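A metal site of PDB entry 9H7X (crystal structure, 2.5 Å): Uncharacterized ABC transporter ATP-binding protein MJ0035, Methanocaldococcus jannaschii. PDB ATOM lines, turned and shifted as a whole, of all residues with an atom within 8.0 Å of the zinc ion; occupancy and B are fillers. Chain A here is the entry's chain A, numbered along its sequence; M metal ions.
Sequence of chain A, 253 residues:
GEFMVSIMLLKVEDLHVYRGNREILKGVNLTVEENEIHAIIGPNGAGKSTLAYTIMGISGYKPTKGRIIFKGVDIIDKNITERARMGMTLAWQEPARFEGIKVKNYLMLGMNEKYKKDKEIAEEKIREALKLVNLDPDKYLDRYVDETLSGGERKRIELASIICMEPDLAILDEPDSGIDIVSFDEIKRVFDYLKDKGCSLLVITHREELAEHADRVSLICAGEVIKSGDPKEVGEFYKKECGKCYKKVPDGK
O of Val 28 is in hydrogen-bond range of N of Asp 14, 3.2 Å away. The backbone carbonyl oxygen (O) of Asp 14 lies close to the backbone NH (N) of Gly 66, 3.5 Å away. The side-chain amide oxygen (OD1) of Asn 29 is in hydrogen-bond range of the backbone NH (N) of Asp 14, 2.9 Å away. A ring nitrogen (ND1) of His 16 sits at hydrogen-bond distance from the side-chain carboxylate (OE2) of Glu 23, at 3.0 Å.
The zinc ion is bound by a ring nitrogen (NE2) of His 16 (2.5 Å), the side-chain carboxylate (OD2) of Asp 14 (2.5 Å) and the side-chain amino group (NZ) of Lys 65 (2.5 Å). The zinc ion has three donor atoms within binding distance.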
ATOM      1  N   ASP A  14     -21.707   7.683 -26.864  1.00  0.00           N
ATOM      2  CA  ASP A  14     -21.695   8.704 -27.928  1.00  0.00           C
ATOM      3  C   ASP A  14     -23.051   8.860 -28.631  1.00  0.00           C
ATOM      4  O   ASP A  14     -23.154   8.713 -29.850  1.00  0.00           O
ATOM      5  CB  ASP A  14     -20.563   8.494 -28.942  1.00  0.00           C
ATOM      6  CG  ASP A  14     -19.822   9.790 -29.246  1.00  0.00           C
ATOM      7  OD1 ASP A  14     -18.808  10.084 -28.570  1.00  0.00           O
ATOM      8  OD2 ASP A  14     -20.282  10.543 -30.150  1.00  0.00           O
ATOM      9  N   LEU A  15     -24.087   9.156 -27.859  1.00  0.00           N
ATOM     10  CA  LEU A  15     -25.441   9.250 -28.379  1.00  0.00           C
ATOM     11  C   LEU A  15     -25.746  10.513 -29.146  1.00  0.00           C
ATOM     12  O   LEU A  15     -25.725  11.601 -28.572  1.00  0.00           O
ATOM     13  CB  LEU A  15     -26.418   9.114 -27.226  1.00  0.00           C
ATOM     14  CG  LEU A  15     -27.772   8.578 -27.609  1.00  0.00           C
ATOM     15  CD1 LEU A  15     -27.683   7.099 -27.941  1.00  0.00           C
ATOM     16  CD2 LEU A  15     -28.766   8.814 -26.512  1.00  0.00           C
ATOM     17  N   HIS A  16     -26.084  10.380 -30.424  1.00  0.00           N
ATOM     18  CA  HIS A  16     -26.490  11.510 -31.253  1.00  0.00           C
ATOM     19  C   HIS A  16     -27.978  11.370 -31.542  1.00  0.00           C
ATOM     20  O   HIS A  16     -28.393  10.355 -32.100  1.00  0.00           O
ATOM     21  CB  HIS A  16     -25.700  11.548 -32.562  1.00  0.00           C
ATOM     22  CG  HIS A  16     -24.274  11.956 -32.409  1.00  0.00           C
ATOM     23  ND1 HIS A  16     -23.853  13.258 -32.628  1.00  0.00           N
ATOM     24  CD2 HIS A  16     -23.186  11.210 -32.083  1.00  0.00           C
ATOM     25  CE1 HIS A  16     -22.551  13.259 -32.431  1.00  0.00           C
ATOM     26  NE2 HIS A  16     -22.103  12.052 -32.099  1.00  0.00           N
ATOM     27  N   GLU A  23     -30.219  18.965 -34.316  1.00  0.00           N
ATOM     28  CA  GLU A  23     -29.482  17.884 -33.668  1.00  0.00           C
ATOM     29  C   GLU A  23     -29.475  18.260 -32.196  1.00  0.00           C
ATOM     30  O   GLU A  23     -28.811  19.221 -31.808  1.00  0.00           O
ATOM     31  CB  GLU A  23     -28.029  17.842 -34.193  1.00  0.00           C
ATOM     32  CG  GLU A  23     -27.151  16.817 -33.491  1.00  0.00           C
ATOM     33  CD  GLU A  23     -25.709  16.806 -33.958  1.00  0.00           C
ATOM     34  OE1 GLU A  23     -25.254  17.855 -34.462  1.00  0.00           O
ATOM     35  OE2 GLU A  23     -25.037  15.766 -33.816  1.00  0.00           O
ATOM     36  N   LEU A  25     -28.988  15.961 -29.238  1.00  0.00           N
ATOM     37  CA  LEU A  25     -27.882  15.341 -28.514  1.00  0.00           C
ATOM     38  C   LEU A  25     -26.708  15.162 -29.459  1.00  0.00           C
ATOM     39  O   LEU A  25     -26.877  14.658 -30.566  1.00  0.00           O
ATOM     40  CB  LEU A  25     -28.308  14.034 -27.866  1.00  0.00           C
ATOM     41  CG  LEU A  25     -29.440  14.159 -26.859  1.00  0.00           C
ATOM     42  CD1 LEU A  25     -29.920  12.793 -26.405  1.00  0.00           C
ATOM     43  CD2 LEU A  25     -29.024  15.014 -25.676  1.00  0.00           C
ATOM     44  N   LYS A  26     -25.539  15.645 -29.074  1.00  0.00           N
ATOM     45  CA  LYS A  26     -24.344  15.582 -29.909  1.00  0.00           C
ATOM     46  C   LYS A  26     -23.256  14.764 -29.198  1.00  0.00           C
ATOM     47  O   LYS A  26     -22.264  15.317 -28.716  1.00  0.00           O
ATOM     48  CB  LYS A  26     -23.814  17.003 -30.228  1.00  0.00           C
ATOM     49  CG  LYS A  26     -24.882  18.074 -30.481  1.00  0.00           C
ATOM     50  CD  LYS A  26     -24.232  19.428 -30.713  1.00  0.00           C
ATOM     51  CE  LYS A  26     -25.214  20.530 -30.995  1.00  0.00           C
ATOM     52  NZ  LYS A  26     -26.098  20.777 -29.843  1.00  0.00           N
ATOM     53  N   GLY A  27     -23.456  13.455 -29.125  1.00  0.00           N
ATOM     54  CA  GLY A  27     -22.493  12.562 -28.494  1.00  0.00           C
ATOM     55  C   GLY A  27     -22.525  12.601 -26.983  1.00  0.00           C
ATOM     56  O   GLY A  27     -21.614  13.153 -26.354  1.00  0.00           O
ATOM     57  N   VAL A  28     -23.549  11.994 -26.379  1.00  0.00           N
ATOM     58  CA  VAL A  28     -23.661  11.958 -24.929  1.00  0.00           C
ATOM     59  C   VAL A  28     -23.025  10.701 -24.384  1.00  0.00           C
ATOM     60  O   VAL A  28     -23.295   9.607 -24.884  1.00  0.00           O
ATOM     61  CB  VAL A  28     -25.130  12.081 -24.474  1.00  0.00           C
ATOM     62  CG1 VAL A  28     -25.241  11.983 -22.959  1.00  0.00           C
ATOM     63  CG2 VAL A  28     -25.754  13.368 -24.983  1.00  0.00           C
ATOM     64  N   ASN A  29     -22.154  10.862 -23.393  1.00  0.00           N
ATOM     65  CA  ASN A  29     -21.502   9.750 -22.716  1.00  0.00           C
ATOM     66  C   ASN A  29     -21.930   9.861 -21.262  1.00  0.00           C
ATOM     67  O   ASN A  29     -21.560  10.808 -20.557  1.00  0.00           O
ATOM     68  CB  ASN A  29     -19.986   9.813 -22.866  1.00  0.00           C
ATOM     69  CG  ASN A  29     -19.542   9.624 -24.294  1.00  0.00           C
ATOM     70  OD1 ASN A  29     -19.779   8.582 -24.910  1.00  0.00           O
ATOM     71  ND2 ASN A  29     -18.903  10.642 -24.850  1.00  0.00           N
ATOM     72  N   LYS A  65     -26.688   8.045 -34.107  1.00  0.00           N
ATOM     73  CA  LYS A  65     -25.394   7.475 -33.773  1.00  0.00           C
ATOM     74  C   LYS A  65     -25.307   7.133 -32.273  1.00  0.00           C
ATOM     75  O   LYS A  65     -26.058   7.678 -31.461  1.00  0.00           O
ATOM     76  CB  LYS A  65     -24.245   8.406 -34.207  1.00  0.00           C
ATOM     77  CG  LYS A  65     -23.041   7.652 -34.772  1.00  0.00           C
ATOM     78  CD  LYS A  65     -21.801   8.511 -34.816  1.00  0.00           C
ATOM     79  CE  LYS A  65     -21.225   8.696 -33.441  1.00  0.00           C
ATOM     80  NZ  LYS A  65     -20.425   9.937 -33.375  1.00  0.00           N
ATOM     81  N   GLY A  66     -24.404   6.208 -31.931  1.00  0.00           N
ATOM     82  CA  GLY A  66     -24.209   5.755 -30.567  1.00  0.00           C
ATOM     83  C   GLY A  66     -25.146   4.642 -30.153  1.00  0.00           C
ATOM     84  O   GLY A  66     -25.844   4.081 -30.994  1.00  0.00           O
ATOM     85  N   GLU A 224     -24.311  17.838 -24.815  1.00  0.00           N
ATOM     86  CA  GLU A 224     -22.993  17.334 -24.434  1.00  0.00           C
ATOM     87  C   GLU A 224     -22.779  17.430 -22.934  1.00  0.00           C
ATOM     88  O   GLU A 224     -23.128  18.450 -22.347  1.00  0.00           O
ATOM     89  CB  GLU A 224     -21.892  18.137 -25.137  1.00  0.00           C
ATOM     90  CG  GLU A 224     -21.407  17.536 -26.436  1.00  0.00           C
ATOM     91  CD  GLU A 224     -20.564  18.481 -27.278  1.00  0.00           C
ATOM     92  OE1 GLU A 224     -19.436  18.099 -27.655  1.00  0.00           O
ATOM     93  OE2 GLU A 224     -21.032  19.614 -27.549  1.00  0.00           O
HETATM   94 ZN    ZN M   1     -19.623  11.926 -32.111  1.00  0.00          ZN
